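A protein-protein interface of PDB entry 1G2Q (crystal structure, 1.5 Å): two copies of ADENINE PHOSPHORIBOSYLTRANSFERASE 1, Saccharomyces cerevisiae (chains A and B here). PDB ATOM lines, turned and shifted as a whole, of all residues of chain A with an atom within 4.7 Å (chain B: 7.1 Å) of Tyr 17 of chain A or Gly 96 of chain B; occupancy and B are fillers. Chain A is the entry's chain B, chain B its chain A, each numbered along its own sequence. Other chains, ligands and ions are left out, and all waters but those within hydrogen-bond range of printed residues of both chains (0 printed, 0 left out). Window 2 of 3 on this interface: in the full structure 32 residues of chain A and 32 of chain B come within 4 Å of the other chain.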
ATOM      1  N   HIS A  15       2.748   1.574  15.866  1.00  0.00           N
ATOM      2  CA  HIS A  15       2.114   2.822  16.249  1.00  0.00           C
ATOM      3  C   HIS A  15       2.716   3.938  15.417  1.00  0.00           C
ATOM      4  O   HIS A  15       3.932   4.112  15.376  1.00  0.00           O
ATOM      5  CB  HIS A  15       2.283   3.137  17.732  1.00  0.00           C
ATOM      6  CG  HIS A  15       1.439   4.290  18.178  1.00  0.00           C
ATOM      7  ND1 HIS A  15       1.764   5.601  17.902  1.00  0.00           N
ATOM      8  CD2 HIS A  15       0.232   4.324  18.790  1.00  0.00           C
ATOM      9  CE1 HIS A  15       0.794   6.391  18.322  1.00  0.00           C
ATOM     10  NE2 HIS A  15      -0.148   5.643  18.865  1.00  0.00           N
ATOM     11  N   GLN A  16       1.855   4.694  14.751  1.00  0.00           N
ATOM     12  CA  GLN A  16       2.300   5.783  13.896  1.00  0.00           C
ATOM     13  C   GLN A  16       2.571   7.074  14.659  1.00  0.00           C
ATOM     14  O   GLN A  16       1.762   7.507  15.481  1.00  0.00           O
ATOM     15  CB  GLN A  16       1.250   6.036  12.817  1.00  0.00           C
ATOM     16  CG  GLN A  16       1.721   6.928  11.694  1.00  0.00           C
ATOM     17  CD  GLN A  16       0.676   7.055  10.610  1.00  0.00           C
ATOM     18  OE1 GLN A  16      -0.343   7.716  10.792  1.00  0.00           O
ATOM     19  NE2 GLN A  16       0.916   6.401   9.478  1.00  0.00           N
ATOM     20  N   TYR A  17       3.718   7.684  14.387  1.00  0.00           N
ATOM     21  CA  TYR A  17       4.087   8.940  15.029  1.00  0.00           C
ATOM     22  C   TYR A  17       4.481   9.985  13.991  1.00  0.00           C
ATOM     23  O   TYR A  17       5.594   9.962  13.470  1.00  0.00           O
ATOM     24  CB  TYR A  17       5.252   8.740  16.006  1.00  0.00           C
ATOM     25  CG  TYR A  17       4.895   8.001  17.282  1.00  0.00           C
ATOM     26  CD1 TYR A  17       5.254   6.666  17.460  1.00  0.00           C
ATOM     27  CD2 TYR A  17       4.201   8.641  18.310  1.00  0.00           C
ATOM     28  CE1 TYR A  17       4.933   5.983  18.636  1.00  0.00           C
ATOM     29  CE2 TYR A  17       3.871   7.967  19.487  1.00  0.00           C
ATOM     30  CZ  TYR A  17       4.242   6.641  19.642  1.00  0.00           C
ATOM     31  OH  TYR A  17       3.918   5.970  20.801  1.00  0.00           O
ATOM     32  N   PRO A  18       3.567  10.912  13.671  1.00  0.00           N
ATOM     33  CA  PRO A  18       3.888  11.947  12.683  1.00  0.00           C
ATOM     34  C   PRO A  18       5.013  12.862  13.166  1.00  0.00           C
ATOM     35  O   PRO A  18       5.186  13.080  14.369  1.00  0.00           O
ATOM     36  CB  PRO A  18       2.571  12.709  12.535  1.00  0.00           C
ATOM     37  CG  PRO A  18       1.533  11.696  12.877  1.00  0.00           C
ATOM     38  CD  PRO A  18       2.144  10.973  14.054  1.00  0.00           C
ATOM     39  N   ASN A  19       5.777  13.393  12.216  1.00  0.00           N
ATOM     40  CA  ASN A  19       6.870  14.308  12.518  1.00  0.00           C
ATOM     41  C   ASN A  19       7.896  13.774  13.512  1.00  0.00           C
ATOM     42  O   ASN A  19       8.287  14.469  14.448  1.00  0.00           O
ATOM     43  CB  ASN A  19       6.293  15.632  13.025  1.00  0.00           C
ATOM     44  CG  ASN A  19       5.272  16.213  12.073  1.00  0.00           C
ATOM     45  OD1 ASN A  19       5.582  16.495  10.914  1.00  0.00           O
ATOM     46  ND2 ASN A  19       4.043  16.384  12.550  1.00  0.00           N
ATOM     47  N   PHE A  20       8.333  12.536  13.306  1.00  0.00           N
ATOM     48  CA  PHE A  20       9.339  11.926  14.172  1.00  0.00           C
ATOM     49  C   PHE A  20      10.272  11.086  13.309  1.00  0.00           C
ATOM     50  O   PHE A  20       9.811  10.331  12.454  1.00  0.00           O
ATOM     51  CB  PHE A  20       8.687  11.023  15.220  1.00  0.00           C
ATOM     52  CG  PHE A  20       9.666  10.456  16.209  1.00  0.00           C
ATOM     53  CD1 PHE A  20      10.009  11.169  17.354  1.00  0.00           C
ATOM     54  CD2 PHE A  20      10.287   9.233  15.972  1.00  0.00           C
ATOM     55  CE1 PHE A  20      10.960  10.671  18.248  1.00  0.00           C
ATOM     56  CE2 PHE A  20      11.236   8.729  16.856  1.00  0.00           C
ATOM     57  CZ  PHE A  20      11.575   9.450  17.997  1.00  0.00           C
ATOM     58  N   ILE A  25       8.420  13.507   8.745  1.00  0.00           N
ATOM     59  CA  ILE A  25       8.661  12.068   8.698  1.00  0.00           C
ATOM     60  C   ILE A  25       7.554  11.294   9.416  1.00  0.00           C
ATOM     61  O   ILE A  25       7.278  11.540  10.588  1.00  0.00           O
ATOM     62  CB  ILE A  25      10.024  11.708   9.335  1.00  0.00           C
ATOM     63  CG1 ILE A  25      11.152  12.446   8.603  1.00  0.00           C
ATOM     64  CG2 ILE A  25      10.251  10.203   9.267  1.00  0.00           C
ATOM     65  CD1 ILE A  25      12.522  12.251   9.223  1.00  0.00           C
ATOM     66  N   LEU A  26       6.908  10.375   8.705  1.00  0.00           N
ATOM     67  CA  LEU A  26       5.845   9.568   9.301  1.00  0.00           C
ATOM     68  C   LEU A  26       6.496   8.310   9.861  1.00  0.00           C
ATOM     69  O   LEU A  26       6.750   7.351   9.134  1.00  0.00           O
ATOM     70  CB  LEU A  26       4.798   9.190   8.252  1.00  0.00           C
ATOM     71  CG  LEU A  26       3.538   8.531   8.817  1.00  0.00           C
ATOM     72  CD1 LEU A  26       2.880   9.480   9.813  1.00  0.00           C
ATOM     73  CD2 LEU A  26       2.574   8.182   7.691  1.00  0.00           C
ATOM     74  N   PHE A  27       6.761   8.327  11.160  1.00  0.00           N
ATOM     75  CA  PHE A  27       7.419   7.215  11.836  1.00  0.00           C
ATOM     76  C   PHE A  27       6.453   6.098  12.218  1.00  0.00           C
ATOM     77  O   PHE A  27       5.278   6.339  12.461  1.00  0.00           O
ATOM     78  CB  PHE A  27       8.102   7.739  13.103  1.00  0.00           C
ATOM     79  CG  PHE A  27       9.128   6.802  13.677  1.00  0.00           C
ATOM     80  CD1 PHE A  27      10.416   6.754  13.154  1.00  0.00           C
ATOM     81  CD2 PHE A  27       8.803   5.953  14.736  1.00  0.00           C
ATOM     82  CE1 PHE A  27      11.368   5.877  13.674  1.00  0.00           C
ATOM     83  CE2 PHE A  27       9.750   5.073  15.261  1.00  0.00           C
ATOM     84  CZ  PHE A  27      11.035   5.035  14.729  1.00  0.00           C
ATOM     85  N   ASP A  29       6.442   2.913  14.939  1.00  0.00           N
ATOM     86  CA  ASP A  29       7.144   2.291  16.061  1.00  0.00           C
ATOM     87  C   ASP A  29       6.833   0.799  16.167  1.00  0.00           C
ATOM     88  O   ASP A  29       5.684   0.416  16.377  1.00  0.00           O
ATOM     89  CB  ASP A  29       6.755   3.027  17.348  1.00  0.00           C
ATOM     90  CG  ASP A  29       7.329   2.386  18.598  1.00  0.00           C
ATOM     91  OD1 ASP A  29       8.387   1.736  18.508  1.00  0.00           O
ATOM     92  OD2 ASP A  29       6.716   2.556  19.683  1.00  0.00           O
ATOM     93  N   LEU B  94      13.606   7.226  21.605  1.00  0.00           N
ATOM     94  CA  LEU B  94      12.286   6.609  21.650  1.00  0.00           C
ATOM     95  C   LEU B  94      11.158   7.524  21.203  1.00  0.00           C
ATOM     96  O   LEU B  94      11.150   8.715  21.515  1.00  0.00           O
ATOM     97  CB  LEU B  94      11.973   6.148  23.079  1.00  0.00           C
ATOM     98  CG  LEU B  94      12.752   4.957  23.622  1.00  0.00           C
ATOM     99  CD1 LEU B  94      12.563   4.840  25.133  1.00  0.00           C
ATOM    100  CD2 LEU B  94      12.270   3.696  22.924  1.00  0.00           C
ATOM    101  N   PRO B  95      10.185   6.975  20.461  1.00  0.00           N
ATOM    102  CA  PRO B  95       9.049   7.776  20.000  1.00  0.00           C
ATOM    103  C   PRO B  95       7.951   7.680  21.063  1.00  0.00           C
ATOM    104  O   PRO B  95       7.973   6.764  21.890  1.00  0.00           O
ATOM    105  CB  PRO B  95       8.652   7.081  18.702  1.00  0.00           C
ATOM    106  CG  PRO B  95       8.891   5.640  19.036  1.00  0.00           C
ATOM    107  CD  PRO B  95      10.225   5.671  19.769  1.00  0.00           C
ATOM    108  N   GLY B  96       7.000   8.609  21.047  1.00  0.00           N
ATOM    109  CA  GLY B  96       5.913   8.562  22.012  1.00  0.00           C
ATOM    110  C   GLY B  96       6.212   9.216  23.349  1.00  0.00           C
ATOM    111  O   GLY B  96       7.325   9.675  23.592  1.00  0.00           O
ATOM    112  N   GLU B  97       5.210   9.264  24.219  1.00  0.00           N
ATOM    113  CA  GLU B  97       5.392   9.865  25.534  1.00  0.00           C
ATOM    114  C   GLU B  97       6.325   8.970  26.344  1.00  0.00           C
ATOM    115  O   GLU B  97       6.141   7.749  26.392  1.00  0.00           O
ATOM    116  CB  GLU B  97       4.040  10.009  26.236  1.00  0.00           C
ATOM    117  CG  GLU B  97       3.021  10.829  25.447  1.00  0.00           C
ATOM    118  CD  GLU B  97       3.353  12.313  25.404  1.00  0.00           C
ATOM    119  OE1 GLU B  97       2.846  13.012  24.499  1.00  0.00           O
ATOM    120  OE2 GLU B  97       4.106  12.787  26.280  1.00  0.00           O
ATOM    121  N   CYS B  98       7.322   9.585  26.976  1.00  0.00           N
ATOM    122  CA  CYS B  98       8.304   8.857  27.773  1.00  0.00           C
ATOM    123  C   CYS B  98       8.529   9.441  29.155  1.00  0.00           C
ATOM    124  O   CYS B  98       8.339  10.635  29.375  1.00  0.00           O
ATOM    125  CB  CYS B  98       9.672   8.865  27.084  1.00  0.00           C
ATOM    126  SG  CYS B  98       9.783   7.965  25.554  1.00  0.00           S
ATOM    127  N   PHE B  99       8.940   8.580  30.078  1.00  0.00           N
ATOM    128  CA  PHE B  99       9.301   9.019  31.413  1.00  0.00           C
ATOM    129  C   PHE B  99      10.804   9.237  31.249  1.00  0.00           C
ATOM    130  O   PHE B  99      11.438   8.597  30.401  1.00  0.00           O
ATOM    131  CB  PHE B  99       9.026   7.929  32.449  1.00  0.00           C
ATOM    132  CG  PHE B  99       7.581   7.812  32.838  1.00  0.00           C
ATOM    133  CD1 PHE B  99       6.937   6.579  32.808  1.00  0.00           C
ATOM    134  CD2 PHE B  99       6.868   8.933  33.255  1.00  0.00           C
ATOM    135  CE1 PHE B  99       5.601   6.459  33.190  1.00  0.00           C
ATOM    136  CE2 PHE B  99       5.528   8.824  33.638  1.00  0.00           C
ATOM    137  CZ  PHE B  99       4.897   7.584  33.604  1.00  0.00           C
ATOM    138  N   GLU B 113      15.288   7.205  29.002  1.00  0.00           N
ATOM    139  CA  GLU B 113      13.837   7.207  28.850  1.00  0.00           C
ATOM    140  C   GLU B 113      13.245   5.808  28.692  1.00  0.00           C
ATOM    141  O   GLU B 113      13.938   4.850  28.341  1.00  0.00           O
ATOM    142  CB  GLU B 113      13.435   8.019  27.611  1.00  0.00           C
ATOM    143  CG  GLU B 113      13.728   9.512  27.668  1.00  0.00           C
ATOM    144  CD  GLU B 113      13.305  10.242  26.401  1.00  0.00           C
ATOM    145  OE1 GLU B 113      13.766   9.857  25.305  1.00  0.00           O
ATOM    146  OE2 GLU B 113      12.516  11.207  26.494  1.00  0.00           O
ATOM    147  N   ILE B 114      11.947   5.713  28.964  1.00  0.00           N
ATOM    148  CA  ILE B 114      11.187   4.483  28.784  1.00  0.00           C
ATOM    149  C   ILE B 114       9.802   4.969  28.347  1.00  0.00           C
ATOM    150  O   ILE B 114       9.334   6.015  28.801  1.00  0.00           O
ATOM    151  CB  ILE B 114      11.097   3.629  30.090  1.00  0.00           C
ATOM    152  CG1 ILE B 114      10.727   2.186  29.733  1.00  0.00           C
ATOM    153  CG2 ILE B 114      10.049   4.204  31.049  1.00  0.00           C
ATOM    154  CD1 ILE B 114      10.921   1.181  30.873  1.00  0.00           C
ATOM    155  N   GLN B 115       9.162   4.248  27.437  1.00  0.00           N
ATOM    156  CA  GLN B 115       7.840   4.659  26.967  1.00  0.00           C
ATOM    157  C   GLN B 115       6.793   4.501  28.068  1.00  0.00           C
ATOM    158  O   GLN B 115       6.701   3.451  28.693  1.00  0.00           O
ATOM    159  CB  GLN B 115       7.452   3.840  25.738  1.00  0.00           C
ATOM    160  CG  GLN B 115       8.336   4.114  24.533  1.00  0.00           C
ATOM    161  CD  GLN B 115       8.072   3.156  23.396  1.00  0.00           C
ATOM    162  OE1 GLN B 115       8.082   1.944  23.590  1.00  0.00           O
ATOM    163  NE2 GLN B 115       7.844   3.693  22.201  1.00  0.00           N
ATOM    164  N   LYS B 116       5.998   5.547  28.290  1.00  0.00           N
ATOM    165  CA  LYS B 116       4.975   5.523  29.335  1.00  0.00           C
ATOM    166  C   LYS B 116       3.945   4.406  29.212  1.00  0.00           C
ATOM    167  O   LYS B 116       3.530   3.831  30.219  1.00  0.00           O
ATOM    168  CB  LYS B 116       4.231   6.862  29.387  1.00  0.00           C
ATOM    169  CG  LYS B 116       5.067   8.041  29.846  1.00  0.00           C
ATOM    170  CD  LYS B 116       4.188   9.274  29.993  1.00  0.00           C
ATOM    171  CE  LYS B 116       4.978  10.469  30.487  1.00  0.00           C
ATOM    172  NZ  LYS B 116       4.081  11.637  30.719  1.00  0.00           N
ATOM    173  N   ASN B 117       3.531   4.098  27.986  1.00  0.00           N
ATOM    174  CA  ASN B 117       2.519   3.066  27.765  1.00  0.00           C
ATOM    175  C   ASN B 117       3.060   1.648  27.602  1.00  0.00           C
ATOM    176  O   ASN B 117       2.287   0.724  27.347  1.00  0.00           O
ATOM    177  CB  ASN B 117       1.686   3.404  26.523  1.00  0.00           C
ATOM    178  CG  ASN B 117       0.870   4.675  26.680  1.00  0.00           C
ATOM    179  OD1 ASN B 117       0.242   5.142  25.723  1.00  0.00           O
ATOM    180  ND2 ASN B 117       0.867   5.239  27.879  1.00  0.00           N
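Of the 11 printed residues of chain B, 4 touch a printed residue of chain A.
Printed residues of chain B that touch a printed residue of chain A: Leu 94, Pro 95, Gly 96 and Gln 115.
Along chain B the printed residues that touch a printed residue of chain A span positions 94 to 115.
Printed residues of chain A that touch a printed residue of chain B: Tyr 17, Phe 20, Phe 27 and Asp 29.
Hydrophobic or aromatic side chains of chain A that line the printed part of chain B: Tyr 17, Phe 20 and Phe 27.
Among the printed residues, 7 pairs touch across the chains.
Among the printed residues, no Asp or Glu carboxylate lies within 4 Å of a Lys or Arg side-chain nitrogen of the other chain.
Tyr 17 of chain A touches Pro 95 of chain B.
CE2 of Tyr 17 of chain A touches CA of Gly 96 of chain B (3.3 Å).
Phe 20 of chain A touches Leu 94 of chain B (CZ to O, 3.6 Å).
CE2 of Phe 20 of chain A touches CB of Pro 95 of chain B, at 3.6 Å.
CG of Pro 95 of chain B touches CE2 of Phe 27 of chain A (3.9 Å).
Pro 95 of chain B touches Asp 29 of chain A.
The side-chain amide nitrogen (NE2) of Gln 115 of chain B sits at hydrogen-bond distance from the side-chain carboxylate (OD2) of Asp 29 of chain A, 3.0 Å away.
No position is printed for both chains.
The backbone NH (N) of Phe 20 of chain A lies within hydrogen-bond range of the backbone carbonyl oxygen (O) of Ile 25 of chain A (3.1 Å).
O of His 15 of chain A is in hydrogen-bond range of N of Asp 29 of chain A, at 2.8 Å.
SG of Cys 98 of chain B is in hydrogen-bond range of O of Gly 96 of chain B (3.6 Å).
The backbone carbonyl oxygen (O) of Phe 27 of chain A sits at hydrogen-bond distance from the backbone NH (N) of Tyr 17 of chain A (2.8 Å).
O of Pro 95 of chain B sits at hydrogen-bond distance from NE2 of Gln 115 of chain B.
Gln 16 of chain A touches none of the printed residues of chain B.
Tyr 17 of chain A touches just these residues of chain B: Pro 95 (3.6 Å) and Gly 96 (3.3 Å).
Of the printed residues of chain B, Asp 29 of chain A touches Pro 95 and Gln 115.
Printed residues of chain A within 4 Å of Pro 95 of chain B: Tyr 17, Phe 20, Phe 27 and Asp 29.
Of the printed residues of chain A, Gly 96 of chain B touches Tyr 17.
Cys 98 of chain B touches none of the printed residues of chain A.
Of the printed residues of chain A, Gln 115 of chain B touches Asp 29 (3.0 Å).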
